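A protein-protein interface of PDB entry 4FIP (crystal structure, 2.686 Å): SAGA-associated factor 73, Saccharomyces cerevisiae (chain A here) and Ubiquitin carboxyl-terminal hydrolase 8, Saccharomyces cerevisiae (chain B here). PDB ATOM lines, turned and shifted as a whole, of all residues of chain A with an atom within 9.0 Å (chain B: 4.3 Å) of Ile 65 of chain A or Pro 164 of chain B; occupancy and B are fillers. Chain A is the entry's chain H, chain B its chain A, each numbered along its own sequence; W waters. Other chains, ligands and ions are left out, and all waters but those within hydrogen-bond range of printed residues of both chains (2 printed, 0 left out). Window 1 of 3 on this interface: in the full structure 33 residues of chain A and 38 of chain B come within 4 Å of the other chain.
OH of Tyr 165 of chain B sits at hydrogen-bond distance from N of Ile 65 of chain A (2.9 Å).
The side-chain amide oxygen (OE1) of Gln 63 of chain A is in hydrogen-bond range of the guanidinium group (NH2) of Arg 168 of chain B (2.8 Å).
Water W2 lies within hydrogen-bond range of O of Tyr 165 of chain B, OE1 of Gln 63 of chain A and NE of Arg 168 of chain B.
Water W1 bridges O of Ile 65 of chain A (2.8 Å) and OH of Tyr 165 of chain B (2.9 Å).
Among the printed residues, pairs that only touch across the chains: Gln 63 of chain A with Tyr 165 of chain B (3.3 Å), Leu 64 of chain A with Tyr 165 of chain B (3.3 Å), Leu 64 of chain A with Arg 168 of chain B (3.97 Å), Ile 65 of chain A with Pro 164 of chain B (3.7 Å), Ile 65 of chain A with Arg 168 of chain B (3.2 Å), Pro 68 of chain A with Pro 164 of chain B (3.9 Å) and Leu 69 of chain A with Pro 164 of chain B (3.98 Å).
Of the 8 printed residues of chain B, 3 touch a printed residue of chain A.
Printed residues of chain B that touch a printed residue of chain A: Pro 164, Tyr 165 and Arg 168.
Hydrophobic or aromatic side chains of chain A that line the printed part of chain B: Ile 65, Pro 68 and Leu 69.
Printed residues of chain B within 4 Å of Leu 64 of chain A: Tyr 165 and Arg 168.
Ile 65 of chain A touches three residues of chain B.
Printed residues of chain B within 4 Å of Pro 68 of chain A: Pro 164.
Of the printed residues of chain B, Leu 69 of chain A touches Pro 164.
No residue of chain A comes within 4 Å of Asn 163 of chain B.
Of the printed residues of chain A, Pro 164 of chain B touches Ile 65 (3.7 Å), Pro 68 (3.9 Å) and Leu 69 (3.98 Å).
Tyr 165 of chain B touches just these residues of chain A: Gln 63, Leu 64 and Ile 65.
Ile 167 of chain B touches none of the printed residues of chain A.
Of the printed residues of chain A, Arg 168 of chain B touches Gln 63, Leu 64 and Ile 65.
The nearest printed residue of chain B that does not touch Ile 65 of chain A is Phe 166 of chain B (6.4 Å).
The nearest printed residue of chain A that does not touch Pro 164 of chain B is Ile 73 of chain A (5.9 Å).
The nearest printed residue of chain B that does not touch Leu 69 of chain A is Ile 419 of chain B (4.1 Å).
N of Tyr 165 of chain B is in hydrogen-bond range of OD1 of Asn 163 of chain B (3.1 Å).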
ATOM      1  N   LEU A  44      21.841 -35.520   5.215  1.00  0.00           N
ATOM      2  CA  LEU A  44      22.159 -35.229   6.596  1.00  0.00           C
ATOM      3  C   LEU A  44      20.900 -35.089   7.495  1.00  0.00           C
ATOM      4  O   LEU A  44      19.996 -34.327   7.183  1.00  0.00           O
ATOM      5  CB  LEU A  44      22.996 -33.948   6.625  1.00  0.00           C
ATOM      6  CG  LEU A  44      23.786 -33.598   7.885  1.00  0.00           C
ATOM      7  CD1 LEU A  44      24.876 -34.617   8.164  1.00  0.00           C
ATOM      8  CD2 LEU A  44      24.380 -32.208   7.740  1.00  0.00           C
ATOM      9  N   TYR A  46      19.415 -34.740  11.692  1.00  0.00           N
ATOM     10  CA  TYR A  46      19.754 -34.207  13.013  1.00  0.00           C
ATOM     11  C   TYR A  46      18.985 -35.016  14.053  1.00  0.00           C
ATOM     12  O   TYR A  46      17.884 -35.479  13.793  1.00  0.00           O
ATOM     13  CB  TYR A  46      19.406 -32.694  13.093  1.00  0.00           C
ATOM     14  CG  TYR A  46      20.025 -31.907  11.950  1.00  0.00           C
ATOM     15  CD1 TYR A  46      21.305 -31.409  12.060  1.00  0.00           C
ATOM     16  CD2 TYR A  46      19.359 -31.734  10.727  1.00  0.00           C
ATOM     17  CE1 TYR A  46      21.906 -30.736  11.008  1.00  0.00           C
ATOM     18  CE2 TYR A  46      19.947 -31.052   9.672  1.00  0.00           C
ATOM     19  CZ  TYR A  46      21.231 -30.564   9.822  1.00  0.00           C
ATOM     20  OH  TYR A  46      21.881 -29.900   8.815  1.00  0.00           O
ATOM     21  N   HIS A  48      17.517 -34.048  16.849  1.00  0.00           N
ATOM     22  CA  HIS A  48      16.347 -33.450  17.418  1.00  0.00           C
ATOM     23  C   HIS A  48      15.965 -32.146  16.782  1.00  0.00           C
ATOM     24  O   HIS A  48      15.624 -31.143  17.435  1.00  0.00           O
ATOM     25  CB  HIS A  48      16.479 -33.378  18.928  1.00  0.00           C
ATOM     26  CG  HIS A  48      17.764 -32.810  19.383  1.00  0.00           C
ATOM     27  ND1 HIS A  48      18.093 -31.530  19.151  1.00  0.00           N
ATOM     28  CD2 HIS A  48      18.817 -33.376  20.098  1.00  0.00           C
ATOM     29  CE1 HIS A  48      19.308 -31.284  19.680  1.00  0.00           C
ATOM     30  NE2 HIS A  48      19.752 -32.420  20.262  1.00  0.00           N
ATOM     31  N   MET A  49      15.971 -32.201  15.463  1.00  0.00           N
ATOM     32  CA  MET A  49      15.342 -31.215  14.639  1.00  0.00           C
ATOM     33  C   MET A  49      14.742 -32.012  13.521  1.00  0.00           C
ATOM     34  O   MET A  49      15.417 -32.374  12.586  1.00  0.00           O
ATOM     35  CB  MET A  49      16.367 -30.225  14.104  1.00  0.00           C
ATOM     36  CG  MET A  49      17.212 -29.565  15.192  1.00  0.00           C
ATOM     37  SD  MET A  49      18.073 -28.109  14.582  1.00  0.00           S
ATOM     38  CE  MET A  49      19.528 -28.782  13.780  1.00  0.00           C
ATOM     39  N   LEU A  54      11.545 -28.792   9.743  1.00  0.00           N
ATOM     40  CA  LEU A  54      12.597 -27.999   9.102  1.00  0.00           C
ATOM     41  C   LEU A  54      12.242 -27.609   7.685  1.00  0.00           C
ATOM     42  O   LEU A  54      12.270 -26.421   7.351  1.00  0.00           O
ATOM     43  CB  LEU A  54      13.898 -28.763   9.069  1.00  0.00           C
ATOM     44  CG  LEU A  54      14.617 -28.976  10.407  1.00  0.00           C
ATOM     45  CD1 LEU A  54      15.797 -29.918  10.192  1.00  0.00           C
ATOM     46  CD2 LEU A  54      15.109 -27.672  11.023  1.00  0.00           C
ATOM     47  N   ALA A  62      18.759 -23.353   4.714  1.00  0.00           N
ATOM     48  CA  ALA A  62      19.126 -23.021   6.078  1.00  0.00           C
ATOM     49  C   ALA A  62      20.418 -23.687   6.462  1.00  0.00           C
ATOM     50  O   ALA A  62      20.616 -24.828   6.170  1.00  0.00           O
ATOM     51  CB  ALA A  62      18.029 -23.508   7.000  1.00  0.00           C
ATOM     52  N   GLN A  63      21.312 -22.999   7.128  1.00  0.00           N
ATOM     53  CA  GLN A  63      22.437 -23.683   7.713  1.00  0.00           C
ATOM     54  C   GLN A  63      21.978 -24.132   9.061  1.00  0.00           C
ATOM     55  O   GLN A  63      21.224 -23.432   9.699  1.00  0.00           O
ATOM     56  CB  GLN A  63      23.629 -22.757   7.901  1.00  0.00           C
ATOM     57  CG  GLN A  63      24.245 -22.253   6.616  1.00  0.00           C
ATOM     58  CD  GLN A  63      25.675 -21.746   6.806  1.00  0.00           C
ATOM     59  OE1 GLN A  63      26.346 -22.088   7.782  1.00  0.00           O
ATOM     60  NE2 GLN A  63      26.137 -20.921   5.882  1.00  0.00           N
ATOM     61  N   LEU A  64      22.453 -25.270   9.533  1.00  0.00           N
ATOM     62  CA  LEU A  64      22.106 -25.702  10.885  1.00  0.00           C
ATOM     63  C   LEU A  64      23.283 -26.354  11.576  1.00  0.00           C
ATOM     64  O   LEU A  64      24.019 -27.098  10.944  1.00  0.00           O
ATOM     65  CB  LEU A  64      20.959 -26.685  10.829  1.00  0.00           C
ATOM     66  CG  LEU A  64      19.685 -26.146  10.195  1.00  0.00           C
ATOM     67  CD1 LEU A  64      18.834 -27.297   9.663  1.00  0.00           C
ATOM     68  CD2 LEU A  64      18.957 -25.273  11.208  1.00  0.00           C
ATOM     69  N   ILE A  65      23.471 -26.019  12.853  1.00  0.00           N
ATOM     70  CA  ILE A  65      24.451 -26.677  13.725  1.00  0.00           C
ATOM     71  C   ILE A  65      23.627 -27.069  14.937  1.00  0.00           C
ATOM     72  O   ILE A  65      23.149 -26.208  15.688  1.00  0.00           O
ATOM     73  CB  ILE A  65      25.612 -25.754  14.162  1.00  0.00           C
ATOM     74  CG1 ILE A  65      26.522 -25.394  12.991  1.00  0.00           C
ATOM     75  CG2 ILE A  65      26.456 -26.365  15.265  1.00  0.00           C
ATOM     76  CD1 ILE A  65      27.351 -24.150  13.275  1.00  0.00           C
ATOM     77  N   GLU A  66      23.416 -28.374  15.092  1.00  0.00           N
ATOM     78  CA  GLU A  66      22.695 -28.908  16.213  1.00  0.00           C
ATOM     79  C   GLU A  66      23.553 -28.756  17.439  1.00  0.00           C
ATOM     80  O   GLU A  66      24.751 -28.926  17.357  1.00  0.00           O
ATOM     81  CB  GLU A  66      22.358 -30.384  15.978  1.00  0.00           C
ATOM     82  CG  GLU A  66      21.301 -30.890  16.959  1.00  0.00           C
ATOM     83  CD  GLU A  66      20.750 -32.239  16.599  1.00  0.00           C
ATOM     84  OE1 GLU A  66      19.528 -32.415  16.723  1.00  0.00           O
ATOM     85  OE2 GLU A  66      21.529 -33.126  16.190  1.00  0.00           O
ATOM     86  N   ASP A  67      22.926 -28.409  18.560  1.00  0.00           N
ATOM     87  CA  ASP A  67      23.609 -28.265  19.855  1.00  0.00           C
ATOM     88  C   ASP A  67      24.940 -27.560  19.753  1.00  0.00           C
ATOM     89  O   ASP A  67      25.951 -28.072  20.211  1.00  0.00           O
ATOM     90  CB  ASP A  67      23.805 -29.623  20.511  1.00  0.00           C
ATOM     91  CG  ASP A  67      22.493 -30.260  20.935  1.00  0.00           C
ATOM     92  OD1 ASP A  67      21.423 -29.627  20.737  1.00  0.00           O
ATOM     93  OD2 ASP A  67      22.535 -31.389  21.479  1.00  0.00           O
ATOM     94  N   PRO A  68      24.940 -26.361  19.176  1.00  0.00           N
ATOM     95  CA  PRO A  68      26.181 -25.663  18.882  1.00  0.00           C
ATOM     96  C   PRO A  68      27.029 -25.229  20.093  1.00  0.00           C
ATOM     97  O   PRO A  68      28.214 -24.967  19.914  1.00  0.00           O
ATOM     98  CB  PRO A  68      25.717 -24.445  18.088  1.00  0.00           C
ATOM     99  CG  PRO A  68      24.335 -24.210  18.534  1.00  0.00           C
ATOM    100  CD  PRO A  68      23.760 -25.558  18.834  1.00  0.00           C
ATOM    101  N   LEU A  69      26.469 -25.144  21.295  1.00  0.00           N
ATOM    102  CA  LEU A  69      27.314 -24.866  22.454  1.00  0.00           C
ATOM    103  C   LEU A  69      27.658 -26.135  23.251  1.00  0.00           C
ATOM    104  O   LEU A  69      28.193 -26.039  24.362  1.00  0.00           O
ATOM    105  CB  LEU A  69      26.683 -23.807  23.362  1.00  0.00           C
ATOM    106  CG  LEU A  69      26.210 -22.488  22.721  1.00  0.00           C
ATOM    107  CD1 LEU A  69      26.421 -21.360  23.714  1.00  0.00           C
ATOM    108  CD2 LEU A  69      26.890 -22.140  21.397  1.00  0.00           C
ATOM    109  N   ASP A  70      27.382 -27.310  22.670  1.00  0.00           N
ATOM    110  CA  ASP A  70      27.646 -28.596  23.329  1.00  0.00           C
ATOM    111  C   ASP A  70      29.118 -28.786  23.725  1.00  0.00           C
ATOM    112  O   ASP A  70      29.418 -29.075  24.897  1.00  0.00           O
ATOM    113  CB  ASP A  70      27.219 -29.772  22.441  1.00  0.00           C
ATOM    114  CG  ASP A  70      27.406 -31.133  23.131  1.00  0.00           C
ATOM    115  OD1 ASP A  70      26.648 -31.433  24.096  1.00  0.00           O
ATOM    116  OD2 ASP A  70      28.304 -31.904  22.699  1.00  0.00           O
ATOM    117  N   LYS A  71      30.019 -28.655  22.749  1.00  0.00           N
ATOM    118  CA  LYS A  71      31.461 -28.707  23.003  1.00  0.00           C
ATOM    119  C   LYS A  71      32.145 -27.511  22.321  1.00  0.00           C
ATOM    120  O   LYS A  71      31.510 -26.828  21.526  1.00  0.00           O
ATOM    121  CB  LYS A  71      32.041 -30.053  22.533  1.00  0.00           C
ATOM    122  CG  LYS A  71      31.761 -30.395  21.075  1.00  0.00           C
ATOM    123  CD  LYS A  71      32.284 -31.780  20.720  1.00  0.00           C
ATOM    124  CE  LYS A  71      32.077 -32.086  19.247  1.00  0.00           C
ATOM    125  NZ  LYS A  71      33.291 -32.724  18.673  1.00  0.00           N
ATOM    126  N   PRO A  72      33.421 -27.223  22.662  1.00  0.00           N
ATOM    127  CA  PRO A  72      34.104 -26.105  22.024  1.00  0.00           C
ATOM    128  C   PRO A  72      34.220 -26.215  20.504  1.00  0.00           C
ATOM    129  O   PRO A  72      34.015 -27.269  19.916  1.00  0.00           O
ATOM    130  CB  PRO A  72      35.501 -26.133  22.660  1.00  0.00           C
ATOM    131  CG  PRO A  72      35.304 -26.768  23.991  1.00  0.00           C
ATOM    132  CD  PRO A  72      34.185 -27.750  23.807  1.00  0.00           C
ATOM    133  N   ILE A  73      34.542 -25.104  19.870  1.00  0.00           N
ATOM    134  CA  ILE A  73      34.729 -25.137  18.434  1.00  0.00           C
ATOM    135  C   ILE A  73      35.947 -26.033  18.213  1.00  0.00           C
ATOM    136  O   ILE A  73      36.942 -25.941  18.909  1.00  0.00           O
ATOM    137  CB  ILE A  73      34.782 -23.714  17.766  1.00  0.00           C
ATOM    138  CG1 ILE A  73      35.453 -23.742  16.362  1.00  0.00           C
ATOM    139  CG2 ILE A  73      35.387 -22.669  18.696  1.00  0.00           C
ATOM    140  CD1 ILE A  73      34.526 -23.963  15.152  1.00  0.00           C
ATOM    141  N   HIS B 162      31.154 -14.695  18.680  1.00  0.00           N
ATOM    142  CA  HIS B 162      30.817 -15.864  19.463  1.00  0.00           C
ATOM    143  C   HIS B 162      29.626 -16.544  18.844  1.00  0.00           C
ATOM    144  O   HIS B 162      29.036 -17.445  19.412  1.00  0.00           O
ATOM    145  CB  HIS B 162      30.627 -15.492  20.933  1.00  0.00           C
ATOM    146  CG  HIS B 162      31.916 -15.178  21.653  1.00  0.00           C
ATOM    147  ND1 HIS B 162      32.522 -13.977  21.574  1.00  0.00           N
ATOM    148  CD2 HIS B 162      32.707 -15.954  22.470  1.00  0.00           C
ATOM    149  CE1 HIS B 162      33.637 -13.976  22.321  1.00  0.00           C
ATOM    150  NE2 HIS B 162      33.760 -15.185  22.860  1.00  0.00           N
ATOM    151  N   ASN B 163      29.285 -16.153  17.631  1.00  0.00           N
ATOM    152  CA  ASN B 163      28.286 -16.858  16.890  1.00  0.00           C
ATOM    153  C   ASN B 163      28.827 -18.087  16.089  1.00  0.00           C
ATOM    154  O   ASN B 163      29.624 -17.952  15.138  1.00  0.00           O
ATOM    155  CB  ASN B 163      27.606 -15.885  15.979  1.00  0.00           C
ATOM    156  CG  ASN B 163      26.443 -16.490  15.301  1.00  0.00           C
ATOM    157  OD1 ASN B 163      26.592 -17.296  14.386  1.00  0.00           O
ATOM    158  ND2 ASN B 163      25.266 -16.153  15.766  1.00  0.00           N
ATOM    159  N   PRO B 164      28.351 -19.282  16.436  1.00  0.00           N
ATOM    160  CA  PRO B 164      28.836 -20.523  15.875  1.00  0.00           C
ATOM    161  C   PRO B 164      28.695 -20.627  14.384  1.00  0.00           C
ATOM    162  O   PRO B 164      29.545 -21.194  13.734  1.00  0.00           O
ATOM    163  CB  PRO B 164      27.947 -21.585  16.506  1.00  0.00           C
ATOM    164  CG  PRO B 164      27.249 -20.925  17.621  1.00  0.00           C
ATOM    165  CD  PRO B 164      27.116 -19.496  17.197  1.00  0.00           C
ATOM    166  N   TYR B 165      27.622 -20.114  13.814  1.00  0.00           N
ATOM    167  CA  TYR B 165      27.532 -20.115  12.330  1.00  0.00           C
ATOM    168  C   TYR B 165      28.588 -19.218  11.690  1.00  0.00           C
ATOM    169  O   TYR B 165      29.214 -19.609  10.701  1.00  0.00           O
ATOM    170  CB  TYR B 165      26.147 -19.699  11.855  1.00  0.00           C
ATOM    171  CG  TYR B 165      25.096 -20.691  12.236  1.00  0.00           C
ATOM    172  CD1 TYR B 165      24.490 -20.661  13.507  1.00  0.00           C
ATOM    173  CD2 TYR B 165      24.694 -21.667  11.343  1.00  0.00           C
ATOM    174  CE1 TYR B 165      23.505 -21.578  13.863  1.00  0.00           C
ATOM    175  CE2 TYR B 165      23.709 -22.577  11.701  1.00  0.00           C
ATOM    176  CZ  TYR B 165      23.131 -22.511  12.956  1.00  0.00           C
ATOM    177  OH  TYR B 165      22.212 -23.428  13.278  1.00  0.00           O
ATOM    178  N   PHE B 166      28.811 -18.037  12.268  1.00  0.00           N
ATOM    179  CA  PHE B 166      29.809 -17.113  11.711  1.00  0.00           C
ATOM    180  C   PHE B 166      31.242 -17.557  11.927  1.00  0.00           C
ATOM    181  O   PHE B 166      32.048 -17.468  11.020  1.00  0.00           O
ATOM    182  CB  PHE B 166      29.671 -15.709  12.265  1.00  0.00           C
ATOM    183  CG  PHE B 166      30.721 -14.781  11.723  1.00  0.00           C
ATOM    184  CD1 PHE B 166      30.608 -14.273  10.439  1.00  0.00           C
ATOM    185  CD2 PHE B 166      31.856 -14.469  12.472  1.00  0.00           C
ATOM    186  CE1 PHE B 166      31.579 -13.436   9.914  1.00  0.00           C
ATOM    187  CE2 PHE B 166      32.820 -13.624  11.964  1.00  0.00           C
ATOM    188  CZ  PHE B 166      32.685 -13.110  10.678  1.00  0.00           C
ATOM    189  N   ILE B 167      31.552 -18.019  13.133  1.00  0.00           N
ATOM    190  CA  ILE B 167      32.858 -18.610  13.382  1.00  0.00           C
ATOM    191  C   ILE B 167      33.165 -19.756  12.418  1.00  0.00           C
ATOM    192  O   ILE B 167      34.237 -19.830  11.851  1.00  0.00           O
ATOM    193  CB  ILE B 167      32.968 -19.196  14.797  1.00  0.00           C
ATOM    194  CG1 ILE B 167      32.941 -18.104  15.838  1.00  0.00           C
ATOM    195  CG2 ILE B 167      34.301 -19.900  14.925  1.00  0.00           C
ATOM    196  CD1 ILE B 167      34.015 -17.049  15.581  1.00  0.00           C
ATOM    197  N   ARG B 168      32.229 -20.678  12.274  1.00  0.00           N
ATOM    198  CA  ARG B 168      32.436 -21.787  11.361  1.00  0.00           C
ATOM    199  C   ARG B 168      32.773 -21.259   9.988  1.00  0.00           C
ATOM    200  O   ARG B 168      33.683 -21.771   9.329  1.00  0.00           O
ATOM    201  CB  ARG B 168      31.204 -22.674  11.269  1.00  0.00           C
ATOM    202  CG  ARG B 168      31.431 -23.938  10.454  1.00  0.00           C
ATOM    203  CD  ARG B 168      30.283 -24.916  10.567  1.00  0.00           C
ATOM    204  NE  ARG B 168      29.150 -24.457   9.780  1.00  0.00           N
ATOM    205  CZ  ARG B 168      28.012 -25.123   9.615  1.00  0.00           C
ATOM    206  NH1 ARG B 168      27.828 -26.290  10.189  1.00  0.00           N
ATOM    207  NH2 ARG B 168      27.051 -24.617   8.859  1.00  0.00           N
ATOM    208  N   ILE B 419      21.957 -17.266  23.287  1.00  0.00           N
ATOM    209  CA  ILE B 419      23.408 -17.263  23.248  1.00  0.00           C
ATOM    210  C   ILE B 419      24.068 -15.863  23.383  1.00  0.00           C
ATOM    211  O   ILE B 419      25.247 -15.776  23.622  1.00  0.00           O
ATOM    212  CB  ILE B 419      23.948 -17.948  21.949  1.00  0.00           C
ATOM    213  CG1 ILE B 419      23.696 -17.090  20.692  1.00  0.00           C
ATOM    214  CG2 ILE B 419      23.412 -19.370  21.801  1.00  0.00           C
ATOM    215  CD1 ILE B 419      24.457 -17.637  19.513  1.00  0.00           C
HETATM  216  O   HOH W   1      21.822 -23.805  16.130  1.00  0.00           O
HETATM  217  O   HOH W   2      28.705 -21.537   9.090  1.00  0.00           O
